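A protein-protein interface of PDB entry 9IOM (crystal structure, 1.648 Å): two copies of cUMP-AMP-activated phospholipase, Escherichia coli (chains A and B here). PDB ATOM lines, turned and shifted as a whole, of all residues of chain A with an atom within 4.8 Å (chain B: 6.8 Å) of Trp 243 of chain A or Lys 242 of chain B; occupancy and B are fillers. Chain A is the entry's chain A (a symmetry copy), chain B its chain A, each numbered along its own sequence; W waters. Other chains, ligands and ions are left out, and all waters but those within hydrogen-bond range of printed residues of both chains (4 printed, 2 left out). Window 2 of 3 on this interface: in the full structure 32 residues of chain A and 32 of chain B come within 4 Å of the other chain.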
ATOM      1  N   PRO A 233      14.214  -8.020   1.691  1.00  0.00           N
ATOM      2  CA  PRO A 233      13.936  -7.587   0.312  1.00  0.00           C
ATOM      3  C   PRO A 233      14.691  -8.383  -0.734  1.00  0.00           C
ATOM      4  O   PRO A 233      14.125  -8.679  -1.792  1.00  0.00           O
ATOM      5  CB  PRO A 233      14.352  -6.107   0.319  1.00  0.00           C
ATOM      6  CG  PRO A 233      14.124  -5.685   1.736  1.00  0.00           C
ATOM      7  CD  PRO A 233      14.519  -6.873   2.570  1.00  0.00           C
ATOM      8  N   LEU A 236      12.618 -11.507  -1.373  1.00  0.00           N
ATOM      9  CA  LEU A 236      11.307 -11.224  -1.953  1.00  0.00           C
ATOM     10  C   LEU A 236      11.435 -10.723  -3.385  1.00  0.00           C
ATOM     11  O   LEU A 236      10.593 -11.038  -4.237  1.00  0.00           O
ATOM     12  CB  LEU A 236      10.561 -10.203  -1.095  1.00  0.00           C
ATOM     13  CG  LEU A 236      10.131 -10.717   0.285  1.00  0.00           C
ATOM     14  CD1 LEU A 236       9.434  -9.604   1.057  1.00  0.00           C
ATOM     15  CD2 LEU A 236       9.246 -11.963   0.159  1.00  0.00           C
ATOM     16  N   MET A 237      12.498  -9.960  -3.669  1.00  0.00           N
ATOM     17  CA  MET A 237      12.723  -9.434  -5.013  1.00  0.00           C
ATOM     18  C   MET A 237      12.887 -10.547  -6.041  1.00  0.00           C
ATOM     19  O   MET A 237      12.616 -10.336  -7.231  1.00  0.00           O
ATOM     20  CB  MET A 237      13.960  -8.531  -5.022  1.00  0.00           C
ATOM     21  CG  MET A 237      13.677  -7.095  -4.590  1.00  0.00           C
ATOM     22  SD  MET A 237      15.169  -6.084  -4.388  1.00  0.00           S
ATOM     23  CE  MET A 237      16.334  -7.119  -5.236  1.00  0.00           C
ATOM     24  N   ALA A 240       8.850 -11.961  -6.408  1.00  0.00           N
ATOM     25  CA  ALA A 240       7.704 -11.060  -6.458  1.00  0.00           C
ATOM     26  C   ALA A 240       8.130  -9.709  -7.004  1.00  0.00           C
ATOM     27  O   ALA A 240       9.045  -9.080  -6.467  1.00  0.00           O
ATOM     28  CB  ALA A 240       7.076 -10.889  -5.070  1.00  0.00           C
ATOM     29  N   LYS A 241       7.445  -9.247  -8.047  1.00  0.00           N
ATOM     30  CA  LYS A 241       7.852  -7.989  -8.654  1.00  0.00           C
ATOM     31  C   LYS A 241       7.494  -6.797  -7.769  1.00  0.00           C
ATOM     32  O   LYS A 241       8.234  -5.805  -7.738  1.00  0.00           O
ATOM     33  CB  LYS A 241       7.231  -7.870 -10.047  1.00  0.00           C
ATOM     34  CG  LYS A 241       7.141  -9.221 -10.792  1.00  0.00           C
ATOM     35  CD  LYS A 241       8.534  -9.794 -11.120  1.00  0.00           C
ATOM     36  CE  LYS A 241       8.579 -11.324 -10.972  1.00  0.00           C
ATOM     37  NZ  LYS A 241       9.909 -11.860 -10.526  1.00  0.00           N
ATOM     38  N   LYS A 242       6.408  -6.890  -7.007  1.00  0.00           N
ATOM     39  CA  LYS A 242       6.015  -5.819  -6.092  1.00  0.00           C
ATOM     40  C   LYS A 242       6.336  -6.230  -4.653  1.00  0.00           C
ATOM     41  O   LYS A 242       5.464  -6.399  -3.791  1.00  0.00           O
ATOM     42  CB  LYS A 242       4.550  -5.475  -6.304  1.00  0.00           C
ATOM     43  CG  LYS A 242       4.367  -4.791  -7.668  1.00  0.00           C
ATOM     44  CD  LYS A 242       2.931  -4.533  -8.021  1.00  0.00           C
ATOM     45  CE  LYS A 242       2.813  -3.862  -9.390  1.00  0.00           C
ATOM     46  NZ  LYS A 242       3.616  -2.610  -9.499  1.00  0.00           N
ATOM     47  N   TRP A 243       7.643  -6.372  -4.406  1.00  0.00           N
ATOM     48  CA  TRP A 243       8.120  -6.938  -3.147  1.00  0.00           C
ATOM     49  C   TRP A 243       7.798  -6.045  -1.951  1.00  0.00           C
ATOM     50  O   TRP A 243       7.612  -6.557  -0.837  1.00  0.00           O
ATOM     51  CB  TRP A 243       9.631  -7.190  -3.221  1.00  0.00           C
ATOM     52  CG  TRP A 243      10.433  -5.928  -3.357  1.00  0.00           C
ATOM     53  CD1 TRP A 243      10.836  -5.335  -4.520  1.00  0.00           C
ATOM     54  CD2 TRP A 243      10.917  -5.089  -2.294  1.00  0.00           C
ATOM     55  NE1 TRP A 243      11.546  -4.191  -4.248  1.00  0.00           N
ATOM     56  CE2 TRP A 243      11.605  -4.016  -2.892  1.00  0.00           C
ATOM     57  CE3 TRP A 243      10.839  -5.145  -0.899  1.00  0.00           C
ATOM     58  CZ2 TRP A 243      12.212  -3.011  -2.147  1.00  0.00           C
ATOM     59  CZ3 TRP A 243      11.437  -4.143  -0.163  1.00  0.00           C
ATOM     60  CH2 TRP A 243      12.118  -3.092  -0.787  1.00  0.00           C
ATOM     61  N   LEU A 244       7.742  -4.724  -2.146  1.00  0.00           N
ATOM     62  CA  LEU A 244       7.461  -3.847  -1.014  1.00  0.00           C
ATOM     63  C   LEU A 244       6.013  -4.002  -0.565  1.00  0.00           C
ATOM     64  O   LEU A 244       5.736  -4.099   0.640  1.00  0.00           O
ATOM     65  CB  LEU A 244       7.774  -2.389  -1.363  1.00  0.00           C
ATOM     66  CG  LEU A 244       7.559  -1.431  -0.184  1.00  0.00           C
ATOM     67  CD1 LEU A 244       8.504  -1.749   0.987  1.00  0.00           C
ATOM     68  CD2 LEU A 244       7.684   0.024  -0.590  1.00  0.00           C
ATOM     69  N   ALA A 245       5.080  -4.070  -1.522  1.00  0.00           N
ATOM     70  CA  ALA A 245       3.692  -4.344  -1.163  1.00  0.00           C
ATOM     71  C   ALA A 245       3.561  -5.697  -0.480  1.00  0.00           C
ATOM     72  O   ALA A 245       2.791  -5.852   0.476  1.00  0.00           O
ATOM     73  CB  ALA A 245       2.794  -4.283  -2.408  1.00  0.00           C
ATOM     74  N   VAL A 246       4.287  -6.699  -0.971  1.00  0.00           N
ATOM     75  CA  VAL A 246       4.254  -8.024  -0.354  1.00  0.00           C
ATOM     76  C   VAL A 246       4.765  -7.963   1.081  1.00  0.00           C
ATOM     77  O   VAL A 246       4.167  -8.541   1.999  1.00  0.00           O
ATOM     78  CB  VAL A 246       5.072  -9.004  -1.213  1.00  0.00           C
ATOM     79  CG1 VAL A 246       5.310 -10.297  -0.479  1.00  0.00           C
ATOM     80  CG2 VAL A 246       4.342  -9.226  -2.535  1.00  0.00           C
ATOM     81  N   GLN A 247       5.864  -7.240   1.300  1.00  0.00           N
ATOM     82  CA  GLN A 247       6.417  -7.156   2.651  1.00  0.00           C
ATOM     83  C   GLN A 247       5.493  -6.375   3.576  1.00  0.00           C
ATOM     84  O   GLN A 247       5.307  -6.745   4.745  1.00  0.00           O
ATOM     85  CB  GLN A 247       7.791  -6.489   2.598  1.00  0.00           C
ATOM     86  CG  GLN A 247       8.597  -6.637   3.883  1.00  0.00           C
ATOM     87  CD  GLN A 247      10.012  -6.114   3.723  1.00  0.00           C
ATOM     88  OE1 GLN A 247      10.214  -4.946   3.380  1.00  0.00           O
ATOM     89  NE2 GLN A 247      11.003  -6.978   3.972  1.00  0.00           N
ATOM     90  N   PHE B 173       8.309   4.043   4.986  1.00  0.00           N
ATOM     91  CA  PHE B 173       8.581   5.300   4.299  1.00  0.00           C
ATOM     92  C   PHE B 173       9.290   6.322   5.184  1.00  0.00           C
ATOM     93  O   PHE B 173       9.944   7.230   4.660  1.00  0.00           O
ATOM     94  CB  PHE B 173       7.272   5.872   3.739  1.00  0.00           C
ATOM     95  CG  PHE B 173       6.564   4.913   2.825  1.00  0.00           C
ATOM     96  CD1 PHE B 173       6.973   4.769   1.510  1.00  0.00           C
ATOM     97  CD2 PHE B 173       5.523   4.125   3.289  1.00  0.00           C
ATOM     98  CE1 PHE B 173       6.332   3.868   0.663  1.00  0.00           C
ATOM     99  CE2 PHE B 173       4.881   3.228   2.452  1.00  0.00           C
ATOM    100  CZ  PHE B 173       5.290   3.095   1.139  1.00  0.00           C
ATOM    101  N   LEU B 236      -1.832   7.425  -8.716  1.00  0.00           N
ATOM    102  CA  LEU B 236      -0.723   7.111  -7.817  1.00  0.00           C
ATOM    103  C   LEU B 236       0.552   6.824  -8.597  1.00  0.00           C
ATOM    104  O   LEU B 236       1.652   7.179  -8.151  1.00  0.00           O
ATOM    105  CB  LEU B 236      -1.085   5.921  -6.930  1.00  0.00           C
ATOM    106  CG  LEU B 236      -2.186   6.202  -5.899  1.00  0.00           C
ATOM    107  CD1 LEU B 236      -2.484   4.938  -5.103  1.00  0.00           C
ATOM    108  CD2 LEU B 236      -1.802   7.372  -4.985  1.00  0.00           C
ATOM    109  N   ALA B 240       4.272   8.235  -7.361  1.00  0.00           N
ATOM    110  CA  ALA B 240       4.887   7.253  -6.475  1.00  0.00           C
ATOM    111  C   ALA B 240       5.312   6.032  -7.270  1.00  0.00           C
ATOM    112  O   ALA B 240       4.492   5.417  -7.956  1.00  0.00           O
ATOM    113  CB  ALA B 240       3.924   6.839  -5.357  1.00  0.00           C
ATOM    114  N   LYS B 241       6.585   5.659  -7.152  1.00  0.00           N
ATOM    115  CA  LYS B 241       7.065   4.537  -7.942  1.00  0.00           C
ATOM    116  C   LYS B 241       6.527   3.208  -7.415  1.00  0.00           C
ATOM    117  O   LYS B 241       6.267   2.289  -8.204  1.00  0.00           O
ATOM    118  CB  LYS B 241       8.594   4.556  -7.980  1.00  0.00           C
ATOM    119  CG  LYS B 241       9.184   5.983  -8.024  1.00  0.00           C
ATOM    120  CD  LYS B 241       8.832   6.714  -9.334  1.00  0.00           C
ATOM    121  CE  LYS B 241       8.547   8.207  -9.104  1.00  0.00           C
ATOM    122  NZ  LYS B 241       7.528   8.791 -10.041  1.00  0.00           N
ATOM    123  N   LYS B 242       6.300   3.101  -6.109  1.00  0.00           N
ATOM    124  CA  LYS B 242       5.739   1.884  -5.523  1.00  0.00           C
ATOM    125  C   LYS B 242       4.272   2.121  -5.156  1.00  0.00           C
ATOM    126  O   LYS B 242       3.857   2.094  -3.990  1.00  0.00           O
ATOM    127  CB  LYS B 242       6.588   1.447  -4.340  1.00  0.00           C
ATOM    128  CG  LYS B 242       7.953   0.942  -4.837  1.00  0.00           C
ATOM    129  CD  LYS B 242       8.909   0.612  -3.728  1.00  0.00           C
ATOM    130  CE  LYS B 242      10.249   0.127  -4.284  1.00  0.00           C
ATOM    131  NZ  LYS B 242      10.110  -1.024  -5.223  1.00  0.00           N
ATOM    132  N   TRP B 243       3.477   2.341  -6.209  1.00  0.00           N
ATOM    133  CA  TRP B 243       2.091   2.768  -6.036  1.00  0.00           C
ATOM    134  C   TRP B 243       1.231   1.695  -5.371  1.00  0.00           C
ATOM    135  O   TRP B 243       0.266   2.032  -4.670  1.00  0.00           O
ATOM    136  CB  TRP B 243       1.487   3.158  -7.391  1.00  0.00           C
ATOM    137  CG  TRP B 243       1.374   2.001  -8.341  1.00  0.00           C
ATOM    138  CD1 TRP B 243       2.299   1.611  -9.269  1.00  0.00           C
ATOM    139  CD2 TRP B 243       0.284   1.071  -8.449  1.00  0.00           C
ATOM    140  NE1 TRP B 243       1.848   0.506  -9.950  1.00  0.00           N
ATOM    141  CE2 TRP B 243       0.619   0.153  -9.463  1.00  0.00           C
ATOM    142  CE3 TRP B 243      -0.941   0.928  -7.791  1.00  0.00           C
ATOM    143  CZ2 TRP B 243      -0.224  -0.888  -9.837  1.00  0.00           C
ATOM    144  CZ3 TRP B 243      -1.773  -0.110  -8.159  1.00  0.00           C
ATOM    145  CH2 TRP B 243      -1.413  -1.002  -9.175  1.00  0.00           C
ATOM    146  N   LEU B 244       1.546   0.414  -5.583  1.00  0.00           N
ATOM    147  CA  LEU B 244       0.725  -0.631  -4.980  1.00  0.00           C
ATOM    148  C   LEU B 244       0.929  -0.665  -3.470  1.00  0.00           C
ATOM    149  O   LEU B 244      -0.044  -0.759  -2.706  1.00  0.00           O
ATOM    150  CB  LEU B 244       1.031  -1.995  -5.606  1.00  0.00           C
ATOM    151  CG  LEU B 244       0.146  -3.120  -5.053  1.00  0.00           C
ATOM    152  CD1 LEU B 244      -1.339  -2.885  -5.372  1.00  0.00           C
ATOM    153  CD2 LEU B 244       0.585  -4.489  -5.533  1.00  0.00           C
ATOM    154  N   ALA B 245       2.184  -0.549  -3.020  1.00  0.00           N
ATOM    155  CA  ALA B 245       2.434  -0.448  -1.585  1.00  0.00           C
ATOM    156  C   ALA B 245       1.758   0.783  -0.998  1.00  0.00           C
ATOM    157  O   ALA B 245       1.215   0.737   0.113  1.00  0.00           O
ATOM    158  CB  ALA B 245       3.944  -0.415  -1.304  1.00  0.00           C
ATOM    159  N   VAL B 246       1.801   1.901  -1.718  1.00  0.00           N
ATOM    160  CA  VAL B 246       1.145   3.121  -1.249  1.00  0.00           C
ATOM    161  C   VAL B 246      -0.358   2.910  -1.120  1.00  0.00           C
ATOM    162  O   VAL B 246      -0.977   3.302  -0.122  1.00  0.00           O
ATOM    163  CB  VAL B 246       1.481   4.277  -2.208  1.00  0.00           C
ATOM    164  CG1 VAL B 246       0.607   5.474  -1.940  1.00  0.00           C
ATOM    165  CG2 VAL B 246       2.964   4.614  -2.072  1.00  0.00           C
ATOM    166  N   GLN B 247      -0.965   2.261  -2.116  1.00  0.00           N
ATOM    167  CA  GLN B 247      -2.409   2.042  -2.063  1.00  0.00           C
ATOM    168  C   GLN B 247      -2.777   1.064  -0.954  1.00  0.00           C
ATOM    169  O   GLN B 247      -3.779   1.252  -0.250  1.00  0.00           O
ATOM    170  CB  GLN B 247      -2.894   1.510  -3.411  1.00  0.00           C
ATOM    171  CG  GLN B 247      -4.407   1.551  -3.581  1.00  0.00           C
ATOM    172  CD  GLN B 247      -4.826   1.179  -4.991  1.00  0.00           C
ATOM    173  OE1 GLN B 247      -4.503   0.091  -5.475  1.00  0.00           O
ATOM    174  NE2 GLN B 247      -5.550   2.084  -5.661  1.00  0.00           N
HETATM  175  O   HOH W   1      12.817  -1.876  -5.892  1.00  0.00           O
HETATM  176  O   HOH W   2       5.631  -0.678  -8.923  1.00  0.00           O
HETATM  177  O   HOH W   3       2.982  -1.443 -12.094  1.00  0.00           O
HETATM  178  O   HOH W   4       8.896  -2.834  -7.059  1.00  0.00           O
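Among the printed residues, merely in contact across the chains: Lys 242 of chain A with Trp 243 of chain B, Lys 242 of chain A with Leu 244 of chain B, Trp 243 of chain A with Lys 242 of chain B, Leu 244 of chain A with Lys 242 of chain B, Leu 244 of chain A with Ala 245 of chain B, Ala 245 of chain A with Leu 244 of chain B and Ala 245 of chain A with Ala 245 of chain B.
Trp 243 of chain A touches one residue of chain B. Of the printed residues of chain B, Lys 242 of chain A touches Trp 243 (3.6 Å) and Leu 244 (3.4 Å). Printed residues of chain B within 4 Å of Leu 244 of chain A: Lys 242 (3.4 Å) and Ala 245 (3.8 Å). Of the printed residues of chain A, Ala 245 of chain B touches Leu 244 and Ala 245. Printed residues of chain A within 4 Å of Trp 243 of chain B: Lys 242 (3.6 Å). Of the printed residues of chain A, Leu 244 of chain B touches Lys 242 (3.4 Å) and Ala 245 (3.8 Å). The nearest printed residue of chain A that does not touch Lys 242 of chain B is Lys 241 of chain A (5.7 Å). The nearest printed residue of chain B that does not touch Ala 245 of chain A is Val 246 of chain B (6.3 Å).
Of the 10 printed residues of chain B, 4 touch a printed residue of chain A. Printed residues of chain B that touch a printed residue of chain A: Lys 242, Trp 243, Leu 244 and Ala 245. Among the printed residues, 7 pairs touch across the chains. Among the printed residues, no Asp or Glu carboxylate lies within 4 Å of a Lys or Arg side-chain nitrogen of the other chain.
Lys 242 of chain A touches Trp 243 of chain B, and with the chains exchanged Trp 243 of chain A touches Lys 242 of chain B. Lys 242 of chain A touches Leu 244 of chain B, and with the chains exchanged Leu 244 of chain A touches Lys 242 of chain B. Leu 244 of chain A touches Ala 245 of chain B, and with the chains exchanged Ala 245 of chain A touches Leu 244 of chain B. Ala 245 of chain A touches its own counterpart, Ala 245 of chain B. 9 positions are printed for both chains.
Water W2 lies within hydrogen-bond range of the side-chain amino group of Lys 242 of chain A (2.9 Å) and the backbone carbonyl oxygen of Lys 241 of chain B (3.1 Å). Water W4 bridges NZ of Lys 242 of chain B and O of Lys 241 of chain A. Water W3 lies within hydrogen-bond range of the side-chain amino group (NZ) of Lys 242 of chain A (2.9 Å) and the indole nitrogen (NE1) of Trp 243 of chain B (3.1 Å). Water W1 bridges NZ of Lys 242 of chain B and NE1 of Trp 243 of chain A.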
